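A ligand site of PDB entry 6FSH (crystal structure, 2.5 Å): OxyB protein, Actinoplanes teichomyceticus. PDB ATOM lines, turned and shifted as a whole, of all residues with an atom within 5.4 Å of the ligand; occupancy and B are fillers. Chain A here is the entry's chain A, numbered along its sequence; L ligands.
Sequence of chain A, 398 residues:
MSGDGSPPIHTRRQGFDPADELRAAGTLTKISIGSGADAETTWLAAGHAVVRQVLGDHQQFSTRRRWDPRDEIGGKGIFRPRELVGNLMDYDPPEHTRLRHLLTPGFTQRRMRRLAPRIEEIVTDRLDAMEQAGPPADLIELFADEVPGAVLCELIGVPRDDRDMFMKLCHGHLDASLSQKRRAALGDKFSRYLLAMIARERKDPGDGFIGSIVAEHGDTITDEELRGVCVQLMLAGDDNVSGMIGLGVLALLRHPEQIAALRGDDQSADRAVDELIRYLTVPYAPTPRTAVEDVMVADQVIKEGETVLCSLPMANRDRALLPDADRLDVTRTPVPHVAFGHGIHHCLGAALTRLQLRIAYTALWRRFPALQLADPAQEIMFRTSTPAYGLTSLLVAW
NE2 of His 96 lies within hydrogen-bond range of ND1 of His 345 (3.3 Å). The backbone NH (N) of Gly 349 lies close to the side-chain sulfur (SG) of Cys 347 (3.0 Å). The backbone NH of Cys 347 sits at hydrogen-bond distance from the backbone carbonyl oxygen of Phe 340 (3.0 Å). The backbone NH (N) of Ala 350 lies close to the side-chain sulfur (SG) of Cys 347 (3.3 Å). The backbone carbonyl oxygen of Thr 287 is in hydrogen-bond range of the guanidinium group of Arg 289. The side-chain hydroxyl (OG1) of Thr 287 sits close to the side-chain sulfur (SD) of Met 89 (3.4 Å). The backbone carbonyl oxygen of Gly 349 is in hydrogen-bond range of the side-chain hydroxyl of Thr 353 (3.0 Å). The backbone carbonyl oxygen (O) of Ala 236 is in hydrogen-bond range of the side-chain amide nitrogen (ND2) of Asn 240.
ND1 of His 345 lies within hydrogen-bond range of O4 of the ligand, 2.4 Å away. SG of Cys 347 binds FE1 of the ligand (2.6 Å). NH1 of Arg 100 is in salt-bridge range of O3 of the ligand (2.6 Å). N of Thr 287 sits at hydrogen-bond distance from O1 of the ligand (2.8 Å). An oxygen (O1) of the ligand is in hydrogen-bond range of the side-chain hydroxyl of Thr 287 (3.1 Å). The guanidinium group (NH1) of Arg 289 lies within salt-bridge range of an oxygen (O1) of the ligand (2.9 Å). A ring nitrogen (NE2) of His 96 lies within hydrogen-bond range of an oxygen (O3) of the ligand (3.0 Å).
Residues that only touch the ligand: Leu 88, Ala 339, Pro 286, Gly 237, Thr 353, Ala 236, Asn 240, Leu 152, Leu 312, Gly 349, Gly 341, Met 244, Phe 340, Pro 283, Leu 155, Met 89, Leu 348, Val 241 and Val 282. Hydrophobic or aromatic side chains within 4 Å of the ligand: Leu 88, Met 89, His 96, Leu 152, Leu 155, Ala 236, Val 241, Met 244, Val 282, Pro 283, Pro 286, Leu 312, Phe 340 and His 345.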
ATOM      1  N   LEU A  55       5.153  10.581  -3.367  1.00  0.00           N
ATOM      2  CA  LEU A  55       5.664   9.251  -3.087  1.00  0.00           C
ATOM      3  C   LEU A  55       5.878   8.419  -4.344  1.00  0.00           C
ATOM      4  O   LEU A  55       6.658   7.459  -4.318  1.00  0.00           O
ATOM      5  CB  LEU A  55       4.700   8.515  -2.172  1.00  0.00           C
ATOM      6  CG  LEU A  55       4.568   9.015  -0.749  1.00  0.00           C
ATOM      7  CD1 LEU A  55       3.457   8.205  -0.037  1.00  0.00           C
ATOM      8  CD2 LEU A  55       5.920   8.855  -0.041  1.00  0.00           C
ATOM      9  N   LEU A  88      16.593   0.349   1.345  1.00  0.00           N
ATOM     10  CA  LEU A  88      15.987   0.676   0.060  1.00  0.00           C
ATOM     11  C   LEU A  88      15.432   2.105   0.050  1.00  0.00           C
ATOM     12  O   LEU A  88      15.361   2.712  -1.013  1.00  0.00           O
ATOM     13  CB  LEU A  88      14.866  -0.319  -0.262  1.00  0.00           C
ATOM     14  CG  LEU A  88      15.158  -1.731  -0.830  1.00  0.00           C
ATOM     15  CD1 LEU A  88      13.914  -2.632  -0.721  1.00  0.00           C
ATOM     16  CD2 LEU A  88      15.689  -1.685  -2.272  1.00  0.00           C
ATOM     17  N   MET A  89      15.096   2.664   1.213  1.00  0.00           N
ATOM     18  CA  MET A  89      14.529   4.004   1.247  1.00  0.00           C
ATOM     19  C   MET A  89      15.558   5.071   0.843  1.00  0.00           C
ATOM     20  O   MET A  89      15.153   6.184   0.500  1.00  0.00           O
ATOM     21  CB  MET A  89      13.961   4.276   2.639  1.00  0.00           C
ATOM     22  CG  MET A  89      12.620   3.523   2.940  1.00  0.00           C
ATOM     23  SD  MET A  89      12.000   3.686   4.674  1.00  0.00           S
ATOM     24  CE  MET A  89      12.681   2.221   5.404  1.00  0.00           C
ATOM     25  N   HIS A  96      17.702   1.333  -6.787  1.00  0.00           N
ATOM     26  CA  HIS A  96      16.579   0.804  -6.017  1.00  0.00           C
ATOM     27  C   HIS A  96      15.975  -0.413  -6.700  1.00  0.00           C
ATOM     28  O   HIS A  96      15.688  -1.423  -6.044  1.00  0.00           O
ATOM     29  CB  HIS A  96      15.504   1.883  -5.841  1.00  0.00           C
ATOM     30  CG  HIS A  96      14.261   1.384  -5.167  1.00  0.00           C
ATOM     31  ND1 HIS A  96      13.179   0.910  -5.859  1.00  0.00           N
ATOM     32  CD2 HIS A  96      13.953   1.270  -3.842  1.00  0.00           C
ATOM     33  CE1 HIS A  96      12.240   0.529  -4.995  1.00  0.00           C
ATOM     34  NE2 HIS A  96      12.690   0.753  -3.775  1.00  0.00           N
ATOM     35  N   ARG A 100      15.650  -4.182  -4.919  1.00  0.00           N
ATOM     36  CA  ARG A 100      14.327  -4.688  -4.560  1.00  0.00           C
ATOM     37  C   ARG A 100      13.979  -5.936  -5.369  1.00  0.00           C
ATOM     38  O   ARG A 100      13.470  -6.909  -4.814  1.00  0.00           O
ATOM     39  CB  ARG A 100      13.280  -3.599  -4.713  1.00  0.00           C
ATOM     40  CG  ARG A 100      11.881  -4.031  -4.292  1.00  0.00           C
ATOM     41  CD  ARG A 100      10.996  -2.830  -4.087  1.00  0.00           C
ATOM     42  NE  ARG A 100       9.605  -3.211  -3.785  1.00  0.00           N
ATOM     43  CZ  ARG A 100       8.856  -2.602  -2.874  1.00  0.00           C
ATOM     44  NH1 ARG A 100       9.353  -1.584  -2.178  1.00  0.00           N
ATOM     45  NH2 ARG A 100       7.610  -2.978  -2.660  1.00  0.00           N
ATOM     46  N   PHE A 107      10.061 -12.796  -0.248  1.00  0.00           N
ATOM     47  CA  PHE A 107       8.741 -12.306   0.123  1.00  0.00           C
ATOM     48  C   PHE A 107       7.618 -12.945  -0.700  1.00  0.00           C
ATOM     49  O   PHE A 107       6.573 -12.345  -0.917  1.00  0.00           O
ATOM     50  CB  PHE A 107       8.683 -10.787  -0.028  1.00  0.00           C
ATOM     51  CG  PHE A 107       9.490 -10.048   1.000  1.00  0.00           C
ATOM     52  CD1 PHE A 107       8.962  -9.797   2.266  1.00  0.00           C
ATOM     53  CD2 PHE A 107      10.776  -9.589   0.706  1.00  0.00           C
ATOM     54  CE1 PHE A 107       9.707  -9.106   3.210  1.00  0.00           C
ATOM     55  CE2 PHE A 107      11.522  -8.911   1.645  1.00  0.00           C
ATOM     56  CZ  PHE A 107      10.997  -8.676   2.896  1.00  0.00           C
ATOM     57  N   LEU A 152       9.920 -11.094  13.308  1.00  0.00           N
ATOM     58  CA  LEU A 152      11.012 -10.722  12.406  1.00  0.00           C
ATOM     59  C   LEU A 152      12.119 -11.760  12.398  1.00  0.00           C
ATOM     60  O   LEU A 152      12.670 -12.064  11.336  1.00  0.00           O
ATOM     61  CB  LEU A 152      11.567  -9.359  12.786  1.00  0.00           C
ATOM     62  CG  LEU A 152      10.698  -8.211  12.275  1.00  0.00           C
ATOM     63  CD1 LEU A 152      10.963  -6.925  13.048  1.00  0.00           C
ATOM     64  CD2 LEU A 152      11.034  -8.044  10.791  1.00  0.00           C
ATOM     65  N   LEU A 155      11.053 -14.375  10.131  1.00  0.00           N
ATOM     66  CA  LEU A 155      11.198 -13.896   8.763  1.00  0.00           C
ATOM     67  C   LEU A 155      12.607 -14.152   8.239  1.00  0.00           C
ATOM     68  O   LEU A 155      12.789 -14.866   7.248  1.00  0.00           O
ATOM     69  CB  LEU A 155      10.894 -12.396   8.694  1.00  0.00           C
ATOM     70  CG  LEU A 155      11.185 -11.794   7.321  1.00  0.00           C
ATOM     71  CD1 LEU A 155      10.152 -12.179   6.260  1.00  0.00           C
ATOM     72  CD2 LEU A 155      11.408 -10.300   7.369  1.00  0.00           C
ATOM     73  N   LEU A 233      15.515  -4.396   8.141  1.00  0.00           N
ATOM     74  CA  LEU A 233      14.202  -5.008   8.369  1.00  0.00           C
ATOM     75  C   LEU A 233      13.866  -5.055   9.858  1.00  0.00           C
ATOM     76  O   LEU A 233      12.723  -4.798  10.257  1.00  0.00           O
ATOM     77  CB  LEU A 233      14.160  -6.427   7.780  1.00  0.00           C
ATOM     78  CG  LEU A 233      14.351  -6.755   6.289  1.00  0.00           C
ATOM     79  CD1 LEU A 233      14.416  -8.274   6.109  1.00  0.00           C
ATOM     80  CD2 LEU A 233      13.240  -6.203   5.400  1.00  0.00           C
ATOM     81  N   ALA A 236      12.655  -1.833  10.527  1.00  0.00           N
ATOM     82  CA  ALA A 236      11.462  -1.413   9.807  1.00  0.00           C
ATOM     83  C   ALA A 236      10.190  -2.013  10.382  1.00  0.00           C
ATOM     84  O   ALA A 236       9.122  -1.388  10.304  1.00  0.00           O
ATOM     85  CB  ALA A 236      11.589  -1.774   8.325  1.00  0.00           C
ATOM     86  N   GLY A 237      10.262  -3.199  10.953  1.00  0.00           N
ATOM     87  CA  GLY A 237       9.048  -3.920  11.283  1.00  0.00           C
ATOM     88  C   GLY A 237       8.739  -4.122  12.742  1.00  0.00           C
ATOM     89  O   GLY A 237       7.918  -4.979  13.099  1.00  0.00           O
ATOM     90  N   ASN A 240       6.701  -0.159  14.306  1.00  0.00           N
ATOM     91  CA  ASN A 240       5.442   0.003  13.598  1.00  0.00           C
ATOM     92  C   ASN A 240       4.392  -1.032  14.051  1.00  0.00           C
ATOM     93  O   ASN A 240       3.230  -0.681  14.273  1.00  0.00           O
ATOM     94  CB  ASN A 240       5.687  -0.086  12.098  1.00  0.00           C
ATOM     95  CG  ASN A 240       6.250   1.225  11.538  1.00  0.00           C
ATOM     96  OD1 ASN A 240       6.018   2.297  12.106  1.00  0.00           O
ATOM     97  ND2 ASN A 240       7.034   1.137  10.454  1.00  0.00           N
ATOM     98  N   VAL A 241       4.788  -2.307  14.170  1.00  0.00           N
ATOM     99  CA  VAL A 241       3.781  -3.330  14.441  1.00  0.00           C
ATOM    100  C   VAL A 241       3.358  -3.301  15.911  1.00  0.00           C
ATOM    101  O   VAL A 241       2.162  -3.321  16.222  1.00  0.00           O
ATOM    102  CB  VAL A 241       4.303  -4.725  14.031  1.00  0.00           C
ATOM    103  CG1 VAL A 241       3.283  -5.807  14.399  1.00  0.00           C
ATOM    104  CG2 VAL A 241       4.644  -4.762  12.521  1.00  0.00           C
ATOM    105  N   MET A 244       0.956  -0.728  16.299  1.00  0.00           N
ATOM    106  CA  MET A 244      -0.349  -1.106  15.768  1.00  0.00           C
ATOM    107  C   MET A 244      -1.129  -2.013  16.731  1.00  0.00           C
ATOM    108  O   MET A 244      -2.351  -1.888  16.855  1.00  0.00           O
ATOM    109  CB  MET A 244      -0.199  -1.749  14.397  1.00  0.00           C
ATOM    110  CG  MET A 244      -0.284  -0.739  13.231  1.00  0.00           C
ATOM    111  SD  MET A 244      -1.742   0.331  13.287  1.00  0.00           S
ATOM    112  CE  MET A 244      -3.069  -0.855  12.918  1.00  0.00           C
ATOM    113  N   ILE A 277      -5.258  -0.094  10.183  1.00  0.00           N
ATOM    114  CA  ILE A 277      -4.028   0.546   9.702  1.00  0.00           C
ATOM    115  C   ILE A 277      -4.322   1.952   9.199  1.00  0.00           C
ATOM    116  O   ILE A 277      -3.626   2.930   9.537  1.00  0.00           O
ATOM    117  CB  ILE A 277      -3.392  -0.338   8.611  1.00  0.00           C
ATOM    118  CG1 ILE A 277      -2.691  -1.522   9.264  1.00  0.00           C
ATOM    119  CG2 ILE A 277      -2.417   0.422   7.734  1.00  0.00           C
ATOM    120  CD1 ILE A 277      -2.734  -2.737   8.424  1.00  0.00           C
ATOM    121  N   VAL A 282       0.119   4.594  11.977  1.00  0.00           N
ATOM    122  CA  VAL A 282       1.097   4.807  13.051  1.00  0.00           C
ATOM    123  C   VAL A 282       2.278   5.687  12.649  1.00  0.00           C
ATOM    124  O   VAL A 282       2.685   6.532  13.460  1.00  0.00           O
ATOM    125  CB  VAL A 282       1.519   3.461  13.660  1.00  0.00           C
ATOM    126  CG1 VAL A 282       0.357   2.775  14.374  1.00  0.00           C
ATOM    127  CG2 VAL A 282       2.126   2.534  12.646  1.00  0.00           C
ATOM    128  N   PRO A 283       2.836   5.602  11.432  1.00  0.00           N
ATOM    129  CA  PRO A 283       3.988   6.462  11.109  1.00  0.00           C
ATOM    130  C   PRO A 283       3.571   7.892  10.777  1.00  0.00           C
ATOM    131  O   PRO A 283       2.589   8.138  10.077  1.00  0.00           O
ATOM    132  CB  PRO A 283       4.625   5.786   9.888  1.00  0.00           C
ATOM    133  CG  PRO A 283       3.883   4.481   9.695  1.00  0.00           C
ATOM    134  CD  PRO A 283       2.523   4.751  10.269  1.00  0.00           C
ATOM    135  N   PRO A 286       6.722   9.396   5.814  1.00  0.00           N
ATOM    136  CA  PRO A 286       7.683   8.520   5.129  1.00  0.00           C
ATOM    137  C   PRO A 286       9.049   9.194   5.021  1.00  0.00           C
ATOM    138  O   PRO A 286       9.289  10.237   5.635  1.00  0.00           O
ATOM    139  CB  PRO A 286       7.033   8.310   3.756  1.00  0.00           C
ATOM    140  CG  PRO A 286       6.376   9.638   3.486  1.00  0.00           C
ATOM    141  CD  PRO A 286       5.886  10.142   4.856  1.00  0.00           C
ATOM    142  N   THR A 287       9.962   8.598   4.243  1.00  0.00           N
ATOM    143  CA  THR A 287      11.265   9.187   4.011  1.00  0.00           C
ATOM    144  C   THR A 287      11.125  10.546   3.342  1.00  0.00           C
ATOM    145  O   THR A 287      10.373  10.671   2.360  1.00  0.00           O
ATOM    146  CB  THR A 287      12.143   8.274   3.156  1.00  0.00           C
ATOM    147  OG1 THR A 287      12.232   6.980   3.786  1.00  0.00           O
ATOM    148  CG2 THR A 287      13.572   8.876   2.959  1.00  0.00           C
ATOM    149  N   ARG A 289      11.499  13.566   0.862  1.00  0.00           N
ATOM    150  CA  ARG A 289      11.798  13.655  -0.554  1.00  0.00           C
ATOM    151  C   ARG A 289      12.485  14.987  -0.861  1.00  0.00           C
ATOM    152  O   ARG A 289      12.249  16.002  -0.193  1.00  0.00           O
ATOM    153  CB  ARG A 289      10.529  13.528  -1.400  1.00  0.00           C
ATOM    154  CG  ARG A 289      10.268  12.141  -1.932  1.00  0.00           C
ATOM    155  CD  ARG A 289       9.786  11.156  -0.845  1.00  0.00           C
ATOM    156  NE  ARG A 289       9.471   9.838  -1.408  1.00  0.00           N
ATOM    157  CZ  ARG A 289       9.325   8.718  -0.695  1.00  0.00           C
ATOM    158  NH1 ARG A 289       9.449   8.736   0.634  1.00  0.00           N
ATOM    159  NH2 ARG A 289       9.044   7.581  -1.312  1.00  0.00           N
ATOM    160  N   LEU A 312       1.405  11.214   6.375  1.00  0.00           N
ATOM    161  CA  LEU A 312       0.546  10.066   6.112  1.00  0.00           C
ATOM    162  C   LEU A 312      -0.739  10.089   6.927  1.00  0.00           C
ATOM    163  O   LEU A 312      -1.778   9.726   6.365  1.00  0.00           O
ATOM    164  CB  LEU A 312       1.325   8.751   6.306  1.00  0.00           C
ATOM    165  CG  LEU A 312       2.658   8.568   5.590  1.00  0.00           C
ATOM    166  CD1 LEU A 312       3.198   7.128   5.789  1.00  0.00           C
ATOM    167  CD2 LEU A 312       2.579   8.961   4.081  1.00  0.00           C
ATOM    168  N   VAL A 338      -2.510   5.467   2.274  1.00  0.00           N
ATOM    169  CA  VAL A 338      -1.059   5.574   2.142  1.00  0.00           C
ATOM    170  C   VAL A 338      -0.299   5.200   3.428  1.00  0.00           C
ATOM    171  O   VAL A 338       0.844   5.628   3.601  1.00  0.00           O
ATOM    172  CB  VAL A 338      -0.637   6.971   1.658  1.00  0.00           C
ATOM    173  CG1 VAL A 338      -1.139   7.193   0.241  1.00  0.00           C
ATOM    174  CG2 VAL A 338      -1.174   8.034   2.598  1.00  0.00           C
ATOM    175  N   ALA A 339      -0.886   4.433   4.357  1.00  0.00           N
ATOM    176  CA  ALA A 339      -0.125   4.067   5.551  1.00  0.00           C
ATOM    177  C   ALA A 339       1.077   3.190   5.233  1.00  0.00           C
ATOM    178  O   ALA A 339       2.058   3.182   5.989  1.00  0.00           O
ATOM    179  CB  ALA A 339      -1.005   3.350   6.589  1.00  0.00           C
ATOM    180  N   PHE A 340       1.041   2.460   4.119  1.00  0.00           N
ATOM    181  CA  PHE A 340       2.177   1.662   3.653  1.00  0.00           C
ATOM    182  C   PHE A 340       2.937   2.378   2.554  1.00  0.00           C
ATOM    183  O   PHE A 340       3.760   1.757   1.853  1.00  0.00           O
ATOM    184  CB  PHE A 340       1.686   0.293   3.136  1.00  0.00           C
ATOM    185  CG  PHE A 340       1.288  -0.681   4.217  1.00  0.00           C
ATOM    186  CD1 PHE A 340       2.150  -0.942   5.292  1.00  0.00           C
ATOM    187  CD2 PHE A 340       0.094  -1.399   4.118  1.00  0.00           C
ATOM    188  CE1 PHE A 340       1.790  -1.874   6.298  1.00  0.00           C
ATOM    189  CE2 PHE A 340      -0.272  -2.325   5.109  1.00  0.00           C
ATOM    190  CZ  PHE A 340       0.587  -2.569   6.199  1.00  0.00           C
ATOM    191  N   GLY A 341       2.652   3.650   2.318  1.00  0.00           N
ATOM    192  CA  GLY A 341       3.262   4.353   1.200  1.00  0.00           C
ATOM    193  C   GLY A 341       2.519   4.058  -0.083  1.00  0.00           C
ATOM    194  O   GLY A 341       1.414   3.534  -0.075  1.00  0.00           O
ATOM    195  N   ILE A 344       6.847   2.731  -5.994  1.00  0.00           N
ATOM    196  CA  ILE A 344       7.979   1.785  -5.979  1.00  0.00           C
ATOM    197  C   ILE A 344       8.421   1.414  -4.571  1.00  0.00           C
ATOM    198  O   ILE A 344       8.905   0.294  -4.339  1.00  0.00           O
ATOM    199  CB  ILE A 344       9.177   2.333  -6.761  1.00  0.00           C
ATOM    200  CG1 ILE A 344       9.547   3.732  -6.252  1.00  0.00           C
ATOM    201  CG2 ILE A 344       8.907   2.281  -8.298  1.00  0.00           C
ATOM    202  CD1 ILE A 344      10.825   4.289  -6.853  1.00  0.00           C
ATOM    203  N   HIS A 345       8.329   2.325  -3.606  1.00  0.00           N
ATOM    204  CA  HIS A 345       8.829   2.064  -2.262  1.00  0.00           C
ATOM    205  C   HIS A 345       7.790   1.430  -1.329  1.00  0.00           C
ATOM    206  O   HIS A 345       8.093   1.252  -0.155  1.00  0.00           O
ATOM    207  CB  HIS A 345       9.333   3.357  -1.633  1.00  0.00           C
ATOM    208  CG  HIS A 345      10.618   3.854  -2.219  1.00  0.00           C
ATOM    209  ND1 HIS A 345      11.844   3.319  -1.897  1.00  0.00           N
ATOM    210  CD2 HIS A 345      10.861   4.875  -3.079  1.00  0.00           C
ATOM    211  CE1 HIS A 345      12.787   3.962  -2.557  1.00  0.00           C
ATOM    212  NE2 HIS A 345      12.225   4.911  -3.280  1.00  0.00           N
ATOM    213  N   HIS A 346       6.601   1.073  -1.829  1.00  0.00           N
ATOM    214  CA  HIS A 346       5.539   0.470  -1.015  1.00  0.00           C
ATOM    215  C   HIS A 346       6.050  -0.591  -0.037  1.00  0.00           C
ATOM    216  O   HIS A 346       6.843  -1.460  -0.411  1.00  0.00           O
ATOM    217  CB  HIS A 346       4.487  -0.126  -1.960  1.00  0.00           C
ATOM    218  CG  HIS A 346       3.264  -0.630  -1.290  1.00  0.00           C
ATOM    219  ND1 HIS A 346       3.137  -1.926  -0.832  1.00  0.00           N
ATOM    220  CD2 HIS A 346       2.088  -0.024  -0.999  1.00  0.00           C
ATOM    221  CE1 HIS A 346       1.948  -2.095  -0.292  1.00  0.00           C
ATOM    222  NE2 HIS A 346       1.288  -0.956  -0.385  1.00  0.00           N
ATOM    223  N   CYS A 347       5.615  -0.490   1.224  1.00  0.00           N
ATOM    224  CA  CYS A 347       6.171  -1.295   2.317  1.00  0.00           C
ATOM    225  C   CYS A 347       6.328  -2.755   1.925  1.00  0.00           C
ATOM    226  O   CYS A 347       5.364  -3.455   1.597  1.00  0.00           O
ATOM    227  CB  CYS A 347       5.276  -1.218   3.568  1.00  0.00           C
ATOM    228  SG  CYS A 347       5.784  -2.433   4.896  1.00  0.00           S
ATOM    229  N   LEU A 348       7.567  -3.222   1.979  1.00  0.00           N
ATOM    230  CA  LEU A 348       7.842  -4.623   1.657  1.00  0.00           C
ATOM    231  C   LEU A 348       7.255  -5.567   2.713  1.00  0.00           C
ATOM    232  O   LEU A 348       7.098  -6.758   2.435  1.00  0.00           O
ATOM    233  CB  LEU A 348       9.359  -4.817   1.543  1.00  0.00           C
ATOM    234  CG  LEU A 348       9.893  -5.725   0.448  1.00  0.00           C
ATOM    235  CD1 LEU A 348       9.278  -5.274  -0.879  1.00  0.00           C
ATOM    236  CD2 LEU A 348      11.421  -5.657   0.428  1.00  0.00           C
ATOM    237  N   GLY A 349       6.949  -5.060   3.916  1.00  0.00           N
ATOM    238  CA  GLY A 349       6.347  -5.822   4.993  1.00  0.00           C
ATOM    239  C   GLY A 349       4.836  -5.801   5.080  1.00  0.00           C
ATOM    240  O   GLY A 349       4.292  -6.342   6.048  1.00  0.00           O
ATOM    241  N   ALA A 350       4.130  -5.222   4.089  1.00  0.00           N
ATOM    242  CA  ALA A 350       2.673  -5.069   4.167  1.00  0.00           C
ATOM    243  C   ALA A 350       1.971  -6.405   4.406  1.00  0.00           C
ATOM    244  O   ALA A 350       1.231  -6.554   5.388  1.00  0.00           O
ATOM    245  CB  ALA A 350       2.137  -4.398   2.901  1.00  0.00           C
ATOM    246  N   LEU A 352       3.057  -9.174   5.513  1.00  0.00           N
ATOM    247  CA  LEU A 352       3.431  -9.707   6.817  1.00  0.00           C
ATOM    248  C   LEU A 352       2.705  -8.988   7.932  1.00  0.00           C
ATOM    249  O   LEU A 352       2.271  -9.609   8.914  1.00  0.00           O
ATOM    250  CB  LEU A 352       4.956  -9.595   7.021  1.00  0.00           C
ATOM    251  CG  LEU A 352       5.510 -10.444   8.166  1.00  0.00           C
ATOM    252  CD1 LEU A 352       5.065 -11.892   8.013  1.00  0.00           C
ATOM    253  CD2 LEU A 352       6.986 -10.367   8.185  1.00  0.00           C
ATOM    254  N   THR A 353       2.575  -7.661   7.821  1.00  0.00           N
ATOM    255  CA  THR A 353       1.869  -6.922   8.855  1.00  0.00           C
ATOM    256  C   THR A 353       0.406  -7.332   8.898  1.00  0.00           C
ATOM    257  O   THR A 353      -0.131  -7.626   9.976  1.00  0.00           O
ATOM    258  CB  THR A 353       1.974  -5.416   8.627  1.00  0.00           C
ATOM    259  OG1 THR A 353       3.362  -5.017   8.592  1.00  0.00           O
ATOM    260  CG2 THR A 353       1.278  -4.688   9.745  1.00  0.00           C
ATOM    261  N   GLN A 356       0.122 -10.892  10.559  1.00  0.00           N
ATOM    262  CA  GLN A 356       0.399 -11.050  11.974  1.00  0.00           C
ATOM    263  C   GLN A 356      -0.583 -10.255  12.831  1.00  0.00           C
ATOM    264  O   GLN A 356      -0.830 -10.623  13.986  1.00  0.00           O
ATOM    265  CB  GLN A 356       1.869 -10.719  12.285  1.00  0.00           C
ATOM    266  CG  GLN A 356       2.250  -9.234  12.407  1.00  0.00           C
ATOM    267  CD  GLN A 356       3.703  -8.986  12.916  1.00  0.00           C
ATOM    268  OE1 GLN A 356       3.964  -8.967  14.143  1.00  0.00           O
ATOM    269  NE2 GLN A 356       4.640  -8.809  11.970  1.00  0.00           N
ATOM    270  N   LEU A 357      -1.095  -9.132  12.292  1.00  0.00           N
ATOM    271  CA  LEU A 357      -2.123  -8.370  12.997  1.00  0.00           C
ATOM    272  C   LEU A 357      -3.438  -9.143  13.058  1.00  0.00           C
ATOM    273  O   LEU A 357      -4.108  -9.148  14.097  1.00  0.00           O
ATOM    274  CB  LEU A 357      -2.342  -7.019  12.313  1.00  0.00           C
ATOM    275  CG  LEU A 357      -1.225  -5.982  12.439  1.00  0.00           C
ATOM    276  CD1 LEU A 357      -1.671  -4.629  11.844  1.00  0.00           C
ATOM    277  CD2 LEU A 357      -0.808  -5.821  13.878  1.00  0.00           C
HETATM  278  C1  LIG L   1       8.553   0.894   3.543  1.00  0.00           C
HETATM  279  C2  LIG L   1       5.036   1.621   6.915  1.00  0.00           C
HETATM  280  C3  LIG L   1       5.947  -2.752   8.673  1.00  0.00           C
HETATM  281  C4  LIG L   1       9.850  -3.211   5.758  1.00  0.00           C
HETATM  282  C5  LIG L   1       7.526   1.443   4.281  1.00  0.00           C
HETATM  283  C6  LIG L   1       6.892   2.709   3.997  1.00  0.00           C
HETATM  284  C7  LIG L   1       5.931   2.893   4.923  1.00  0.00           C
HETATM  285  C8  LIG L   1       5.912   1.763   5.836  1.00  0.00           C
HETATM  286  C9  LIG L   1       4.988   4.115   5.027  1.00  0.00           C
HETATM  287  C10 LIG L   1       7.242   3.660   2.815  1.00  0.00           C
HETATM  288  C11 LIG L   1       8.593   4.353   3.028  1.00  0.00           C
HETATM  289  C12 LIG L   1       8.767   5.543   2.116  1.00  0.00           C
HETATM  290  O1  LIG L   1       9.482   6.512   2.463  1.00  0.00           O
HETATM  291  O2  LIG L   1       8.168   5.563   1.014  1.00  0.00           O
HETATM  292  C13 LIG L   1       4.855   0.483   7.683  1.00  0.00           C
HETATM  293  C14 LIG L   1       3.790   0.142   8.645  1.00  0.00           C
HETATM  294  C15 LIG L   1       4.084  -1.086   9.108  1.00  0.00           C
HETATM  295  C16 LIG L   1       5.302  -1.538   8.475  1.00  0.00           C
HETATM  296  C17 LIG L   1       2.572   1.057   9.031  1.00  0.00           C
HETATM  297  C18 LIG L   1       3.366  -1.990  10.150  1.00  0.00           C
HETATM  298  C19 LIG L   1       2.454  -1.535  11.009  1.00  0.00           C
HETATM  299  C20 LIG L   1       7.063  -3.249   8.035  1.00  0.00           C
HETATM  300  C21 LIG L   1       7.632  -4.569   8.248  1.00  0.00           C
HETATM  301  C22 LIG L   1       8.716  -4.704   7.453  1.00  0.00           C
HETATM  302  C23 LIG L   1       8.844  -3.472   6.690  1.00  0.00           C
HETATM  303  C24 LIG L   1       7.027  -5.598   9.246  1.00  0.00           C
HETATM  304  C25 LIG L   1       9.673  -5.916   7.292  1.00  0.00           C
HETATM  305  C26 LIG L   1       9.419  -7.139   7.768  1.00  0.00           C
HETATM  306  C27 LIG L   1       9.888  -2.116   4.897  1.00  0.00           C
HETATM  307  C28 LIG L   1      10.891  -1.780   3.934  1.00  0.00           C
HETATM  308  C29 LIG L   1      10.542  -0.661   3.314  1.00  0.00           C
HETATM  309  C30 LIG L   1       9.288  -0.232   3.881  1.00  0.00           C
HETATM  310  C31 LIG L   1      12.163  -2.572   3.631  1.00  0.00           C
HETATM  311  C32 LIG L   1      11.341   0.040   2.186  1.00  0.00           C
HETATM  312  C33 LIG L   1      10.645  -0.346   0.874  1.00  0.00           C
HETATM  313  C34 LIG L   1      11.400   0.222  -0.332  1.00  0.00           C
HETATM  314  O3  LIG L   1      11.573  -0.576  -1.291  1.00  0.00           O
HETATM  315  O4  LIG L   1      11.824   1.414  -0.400  1.00  0.00           O
HETATM  316  N1  LIG L   1       6.916   0.871   5.400  1.00  0.00           N
HETATM  317  N2  LIG L   1       5.737  -0.564   7.625  1.00  0.00           N
HETATM  318  N3  LIG L   1       7.803  -2.611   7.063  1.00  0.00           N
HETATM  319  N4  LIG L   1       8.918  -1.134   4.850  1.00  0.00           N
HETATM  320 FE1  LIG L   1       7.308  -0.830   6.170  1.00  0.00          FE
